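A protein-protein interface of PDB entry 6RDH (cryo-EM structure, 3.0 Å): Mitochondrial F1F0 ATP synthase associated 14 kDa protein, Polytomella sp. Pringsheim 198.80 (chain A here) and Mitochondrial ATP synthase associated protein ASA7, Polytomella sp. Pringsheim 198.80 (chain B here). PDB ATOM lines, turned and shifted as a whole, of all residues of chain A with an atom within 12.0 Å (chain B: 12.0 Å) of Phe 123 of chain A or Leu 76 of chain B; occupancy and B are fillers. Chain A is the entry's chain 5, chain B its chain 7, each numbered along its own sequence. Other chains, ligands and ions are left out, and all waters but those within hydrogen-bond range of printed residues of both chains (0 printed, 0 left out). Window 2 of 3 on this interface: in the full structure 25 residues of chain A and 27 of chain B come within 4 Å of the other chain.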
ATOM      1  N   ILE A 115      19.909   6.964   4.815  1.00  0.00           N
ATOM      2  CA  ILE A 115      18.821   7.920   4.658  1.00  0.00           C
ATOM      3  C   ILE A 115      19.170   9.237   5.340  1.00  0.00           C
ATOM      4  O   ILE A 115      18.773  10.307   4.873  1.00  0.00           O
ATOM      5  CB  ILE A 115      17.501   7.307   5.160  1.00  0.00           C
ATOM      6  CG1 ILE A 115      16.328   8.274   5.017  1.00  0.00           C
ATOM      7  CG2 ILE A 115      17.618   6.840   6.586  1.00  0.00           C
ATOM      8  CD1 ILE A 115      16.070   8.709   3.607  1.00  0.00           C
ATOM      9  N   TRP A 116      19.966   9.207   6.400  1.00  0.00           N
ATOM     10  CA  TRP A 116      20.325  10.436   7.088  1.00  0.00           C
ATOM     11  C   TRP A 116      21.536  11.119   6.485  1.00  0.00           C
ATOM     12  O   TRP A 116      21.889  12.214   6.923  1.00  0.00           O
ATOM     13  CB  TRP A 116      20.552  10.147   8.568  1.00  0.00           C
ATOM     14  CG  TRP A 116      19.458   9.314   9.118  1.00  0.00           C
ATOM     15  CD1 TRP A 116      19.524   8.008   9.470  1.00  0.00           C
ATOM     16  CD2 TRP A 116      18.109   9.721   9.338  1.00  0.00           C
ATOM     17  NE1 TRP A 116      18.307   7.576   9.911  1.00  0.00           N
ATOM     18  CE2 TRP A 116      17.418   8.613   9.835  1.00  0.00           C
ATOM     19  CE3 TRP A 116      17.421  10.922   9.170  1.00  0.00           C
ATOM     20  CZ2 TRP A 116      16.077   8.665  10.170  1.00  0.00           C
ATOM     21  CZ3 TRP A 116      16.093  10.973   9.493  1.00  0.00           C
ATOM     22  CH2 TRP A 116      15.431   9.854   9.993  1.00  0.00           C
ATOM     23  N   LYS A 119      18.836  12.481   2.685  1.00  0.00           N
ATOM     24  CA  LYS A 119      17.818  13.443   3.083  1.00  0.00           C
ATOM     25  C   LYS A 119      18.083  13.689   4.554  1.00  0.00           C
ATOM     26  O   LYS A 119      17.589  12.932   5.399  1.00  0.00           O
ATOM     27  CB  LYS A 119      16.408  12.899   2.860  1.00  0.00           C
ATOM     28  CG  LYS A 119      15.964  12.928   1.420  1.00  0.00           C
ATOM     29  CD  LYS A 119      15.947  14.349   0.916  1.00  0.00           C
ATOM     30  CE  LYS A 119      15.313  14.453  -0.451  1.00  0.00           C
ATOM     31  NZ  LYS A 119      13.882  14.048  -0.421  1.00  0.00           N
ATOM     32  N   PRO A 120      18.866  14.737   4.910  1.00  0.00           N
ATOM     33  CA  PRO A 120      19.634  14.723   6.165  1.00  0.00           C
ATOM     34  C   PRO A 120      18.844  14.626   7.459  1.00  0.00           C
ATOM     35  O   PRO A 120      18.962  13.602   8.137  1.00  0.00           O
ATOM     36  CB  PRO A 120      20.413  16.042   6.099  1.00  0.00           C
ATOM     37  CG  PRO A 120      19.754  16.846   5.085  1.00  0.00           C
ATOM     38  CD  PRO A 120      19.183  15.917   4.098  1.00  0.00           C
ATOM     39  N   ALA A 121      18.047  15.649   7.779  1.00  0.00           N
ATOM     40  CA  ALA A 121      16.989  15.666   8.788  1.00  0.00           C
ATOM     41  C   ALA A 121      16.377  17.049   8.758  1.00  0.00           C
ATOM     42  O   ALA A 121      16.799  17.895   7.972  1.00  0.00           O
ATOM     43  CB  ALA A 121      17.464  15.382  10.212  1.00  0.00           C
ATOM     44  N   LEU A 122      15.392  17.291   9.611  1.00  0.00           N
ATOM     45  CA  LEU A 122      15.008  18.653   9.970  1.00  0.00           C
ATOM     46  C   LEU A 122      14.673  18.633  11.459  1.00  0.00           C
ATOM     47  O   LEU A 122      13.573  18.288  11.878  1.00  0.00           O
ATOM     48  CB  LEU A 122      13.839  19.181   9.147  1.00  0.00           C
ATOM     49  CG  LEU A 122      14.173  19.979   7.908  1.00  0.00           C
ATOM     50  CD1 LEU A 122      12.923  20.240   7.133  1.00  0.00           C
ATOM     51  CD2 LEU A 122      14.747  21.257   8.386  1.00  0.00           C
ATOM     52  N   PHE A 123      15.649  18.987  12.276  1.00  0.00           N
ATOM     53  CA  PHE A 123      15.366  19.099  13.688  1.00  0.00           C
ATOM     54  C   PHE A 123      15.355  20.583  14.018  1.00  0.00           C
ATOM     55  O   PHE A 123      14.627  21.024  14.899  1.00  0.00           O
ATOM     56  CB  PHE A 123      16.394  18.358  14.543  1.00  0.00           C
ATOM     57  CG  PHE A 123      15.936  18.113  15.958  1.00  0.00           C
ATOM     58  CD1 PHE A 123      15.247  16.954  16.284  1.00  0.00           C
ATOM     59  CD2 PHE A 123      16.123  19.070  16.947  1.00  0.00           C
ATOM     60  CE1 PHE A 123      14.809  16.727  17.590  1.00  0.00           C
ATOM     61  CE2 PHE A 123      15.682  18.856  18.244  1.00  0.00           C
ATOM     62  CZ  PHE A 123      15.023  17.686  18.563  1.00  0.00           C
ATOM     63  N   LEU B  15      11.144  34.115   9.520  1.00  0.00           N
ATOM     64  CA  LEU B  15      10.074  34.985   9.067  1.00  0.00           C
ATOM     65  C   LEU B  15      10.073  36.281   9.872  1.00  0.00           C
ATOM     66  O   LEU B  15      10.978  36.523  10.667  1.00  0.00           O
ATOM     67  CB  LEU B  15       8.713  34.277   9.145  1.00  0.00           C
ATOM     68  CG  LEU B  15       8.061  33.877  10.474  1.00  0.00           C
ATOM     69  CD1 LEU B  15       6.582  33.752  10.298  1.00  0.00           C
ATOM     70  CD2 LEU B  15       8.577  32.548  10.949  1.00  0.00           C
ATOM     71  N   SER B  72       7.706  33.506  19.307  1.00  0.00           N
ATOM     72  CA  SER B  72       8.972  32.817  19.144  1.00  0.00           C
ATOM     73  C   SER B  72       8.920  32.017  17.853  1.00  0.00           C
ATOM     74  O   SER B  72       7.849  31.613  17.398  1.00  0.00           O
ATOM     75  CB  SER B  72       9.265  31.893  20.323  1.00  0.00           C
ATOM     76  OG  SER B  72      10.261  30.949  19.975  1.00  0.00           O
ATOM     77  N   LYS B  73      10.077  31.824  17.243  1.00  0.00           N
ATOM     78  CA  LYS B  73      10.155  31.081  15.998  1.00  0.00           C
ATOM     79  C   LYS B  73      10.814  29.736  16.247  1.00  0.00           C
ATOM     80  O   LYS B  73      11.690  29.602  17.105  1.00  0.00           O
ATOM     81  CB  LYS B  73      10.942  31.852  14.941  1.00  0.00           C
ATOM     82  CG  LYS B  73      10.539  33.293  14.798  1.00  0.00           C
ATOM     83  CD  LYS B  73       9.078  33.426  14.473  1.00  0.00           C
ATOM     84  CE  LYS B  73       8.721  34.865  14.205  1.00  0.00           C
ATOM     85  NZ  LYS B  73       9.540  35.457  13.122  1.00  0.00           N
ATOM     86  N   ILE B  74      10.378  28.732  15.491  1.00  0.00           N
ATOM     87  CA  ILE B  74      11.025  27.430  15.573  1.00  0.00           C
ATOM     88  C   ILE B  74      12.384  27.477  14.890  1.00  0.00           C
ATOM     89  O   ILE B  74      13.399  27.083  15.480  1.00  0.00           O
ATOM     90  CB  ILE B  74      10.118  26.339  14.983  1.00  0.00           C
ATOM     91  CG1 ILE B  74       8.924  26.115  15.899  1.00  0.00           C
ATOM     92  CG2 ILE B  74      10.863  25.040  14.854  1.00  0.00           C
ATOM     93  CD1 ILE B  74       9.316  25.662  17.278  1.00  0.00           C
ATOM     94  N   SER B  75      12.420  27.993  13.655  1.00  0.00           N
ATOM     95  CA  SER B  75      13.626  28.171  12.839  1.00  0.00           C
ATOM     96  C   SER B  75      14.346  26.834  12.633  1.00  0.00           C
ATOM     97  O   SER B  75      15.417  26.573  13.178  1.00  0.00           O
ATOM     98  CB  SER B  75      14.562  29.232  13.428  1.00  0.00           C
ATOM     99  OG  SER B  75      15.465  29.706  12.448  1.00  0.00           O
ATOM    100  N   LEU B  76      13.671  25.973  11.875  1.00  0.00           N
ATOM    101  CA  LEU B  76      14.158  24.628  11.615  1.00  0.00           C
ATOM    102  C   LEU B  76      15.436  24.658  10.803  1.00  0.00           C
ATOM    103  O   LEU B  76      15.612  25.496   9.917  1.00  0.00           O
ATOM    104  CB  LEU B  76      13.109  23.828  10.860  1.00  0.00           C
ATOM    105  CG  LEU B  76      11.956  23.367  11.724  1.00  0.00           C
ATOM    106  CD1 LEU B  76      10.898  22.796  10.857  1.00  0.00           C
ATOM    107  CD2 LEU B  76      12.449  22.342  12.700  1.00  0.00           C
ATOM    108  N   ALA B  77      16.335  23.733  11.110  1.00  0.00           N
ATOM    109  CA  ALA B  77      17.587  23.622  10.391  1.00  0.00           C
ATOM    110  C   ALA B  77      17.978  22.163  10.311  1.00  0.00           C
ATOM    111  O   ALA B  77      17.725  21.384  11.229  1.00  0.00           O
ATOM    112  CB  ALA B  77      18.694  24.416  11.060  1.00  0.00           C
ATOM    113  N   GLU B  78      18.615  21.809   9.209  1.00  0.00           N
ATOM    114  CA  GLU B  78      18.918  20.427   8.902  1.00  0.00           C
ATOM    115  C   GLU B  78      20.206  20.016   9.585  1.00  0.00           C
ATOM    116  O   GLU B  78      21.205  20.733   9.527  1.00  0.00           O
ATOM    117  CB  GLU B  78      19.039  20.257   7.392  1.00  0.00           C
ATOM    118  CG  GLU B  78      18.003  21.056   6.650  1.00  0.00           C
ATOM    119  CD  GLU B  78      18.171  21.005   5.159  1.00  0.00           C
ATOM    120  OE1 GLU B  78      18.653  19.977   4.655  1.00  0.00           O
ATOM    121  OE2 GLU B  78      17.814  21.992   4.487  1.00  0.00           O
ATOM    122  N   VAL B  79      20.179  18.866  10.248  1.00  0.00           N
ATOM    123  CA  VAL B  79      21.399  18.278  10.778  1.00  0.00           C
ATOM    124  C   VAL B  79      21.871  17.245   9.756  1.00  0.00           C
ATOM    125  O   VAL B  79      21.163  16.303   9.402  1.00  0.00           O
ATOM    126  CB  VAL B  79      21.219  17.728  12.198  1.00  0.00           C
ATOM    127  CG1 VAL B  79      20.867  18.872  13.108  1.00  0.00           C
ATOM    128  CG2 VAL B  79      20.127  16.718  12.334  1.00  0.00           C
ATOM    129  N   ALA B  80      23.035  17.497   9.185  1.00  0.00           N
ATOM    130  CA  ALA B  80      23.562  16.684   8.108  1.00  0.00           C
ATOM    131  C   ALA B  80      24.829  15.986   8.564  1.00  0.00           C
ATOM    132  O   ALA B  80      25.434  16.352   9.570  1.00  0.00           O
ATOM    133  CB  ALA B  80      23.841  17.542   6.882  1.00  0.00           C
ATOM    134  N   ARG B  81      25.217  14.954   7.821  1.00  0.00           N
ATOM    135  CA  ARG B  81      26.411  14.210   8.194  1.00  0.00           C
ATOM    136  C   ARG B  81      27.658  15.023   7.916  1.00  0.00           C
ATOM    137  O   ARG B  81      28.575  15.074   8.739  1.00  0.00           O
ATOM    138  CB  ARG B  81      26.468  12.882   7.451  1.00  0.00           C
ATOM    139  CG  ARG B  81      27.701  12.081   7.758  1.00  0.00           C
ATOM    140  CD  ARG B  81      27.563  10.690   7.242  1.00  0.00           C
ATOM    141  NE  ARG B  81      28.789   9.923   7.371  1.00  0.00           N
ATOM    142  CZ  ARG B  81      29.615   9.680   6.367  1.00  0.00           C
ATOM    143  NH1 ARG B  81      30.709   8.966   6.562  1.00  0.00           N
ATOM    144  NH2 ARG B  81      29.343  10.158   5.164  1.00  0.00           N
ATOM    145  N   VAL B  84      24.815  20.277   3.964  1.00  0.00           N
ATOM    146  CA  VAL B  84      23.589  20.174   3.186  1.00  0.00           C
ATOM    147  C   VAL B  84      23.903  20.160   1.701  1.00  0.00           C
ATOM    148  O   VAL B  84      23.218  19.487   0.921  1.00  0.00           O
ATOM    149  CB  VAL B  84      22.646  21.320   3.570  1.00  0.00           C
ATOM    150  CG1 VAL B  84      21.312  21.160   2.923  1.00  0.00           C
ATOM    151  CG2 VAL B  84      22.470  21.339   5.058  1.00  0.00           C
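N of Phe 123 of chain A sits at hydrogen-bond distance from O of Ala 77 of chain B (3.3 Å).
CG of Pro 120 of chain A touches OE1 of Glu 78 of chain B (3.3 Å). Pro 120 of chain A touches Val 79 of chain B (CB to O, 3.4 Å). Ala 80 of chain B touches Pro 120 of chain A (CA to CB, 3.8 Å). Glu 78 of chain B touches Ala 121 of chain A (CB to O, 3.3 Å). Ala 121 of chain A touches Val 79 of chain B. Leu 122 of chain A touches Leu 76 of chain B. Leu 122 of chain A touches Ala 77 of chain B (CD2 to C, 3.9 Å). Leu 122 of chain A touches Glu 78 of chain B. Leu 76 of chain B touches Phe 123 of chain A (CD2 to O, 3.4 Å).
Lys 119 of chain A touches none of the printed residues of chain B. Printed residues of chain B within 4 Å of Pro 120 of chain A: Glu 78, Val 79 and Ala 80. Printed residues of chain B within 4 Å of Ala 121 of chain A: Glu 78 (3.3 Å) and Val 79 (3.6 Å). Of chain B, only Leu 76, Ala 77 and Glu 78 come within 4 Å of Leu 122 of chain A. Phe 123 of chain A touches just these residues of chain B: Leu 76 (3.4 Å) and Ala 77 (3.3 Å). No residue of chain A comes within 4 Å of Ile 74 of chain B. No residue of chain A comes within 4 Å of Ser 75 of chain B. Leu 76 of chain B touches just these residues of chain A: Leu 122 (3.9 Å) and Phe 123 (3.4 Å). Of chain A, only Leu 122 and Phe 123 come within 4 Å of Ala 77 of chain B. Of the printed residues of chain A, Glu 78 of chain B touches Pro 120 (3.3 Å), Ala 121 (3.3 Å) and Leu 122 (3.7 Å). Val 79 of chain B touches just these residues of chain A: Pro 120 (3.4 Å) and Ala 121 (3.6 Å). Of the printed residues of chain A, Ala 80 of chain B touches Pro 120 (3.8 Å). Val 84 of chain B touches none of the printed residues of chain A.
Printed residues of chain B that touch a printed residue of chain A: Leu 76, Ala 77, Glu 78, Val 79 and Ala 80. Hydrophobic or aromatic side chains of chain B that line the printed part of chain A: Leu 76, Val 79 and Ala 80. Of the 7 printed residues of chain A, 4 touch a printed residue of chain B. Hydrophobic or aromatic side chains of chain A within 4 Å of the printed part of chain B: Pro 120, Ala 121 and Leu 122.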
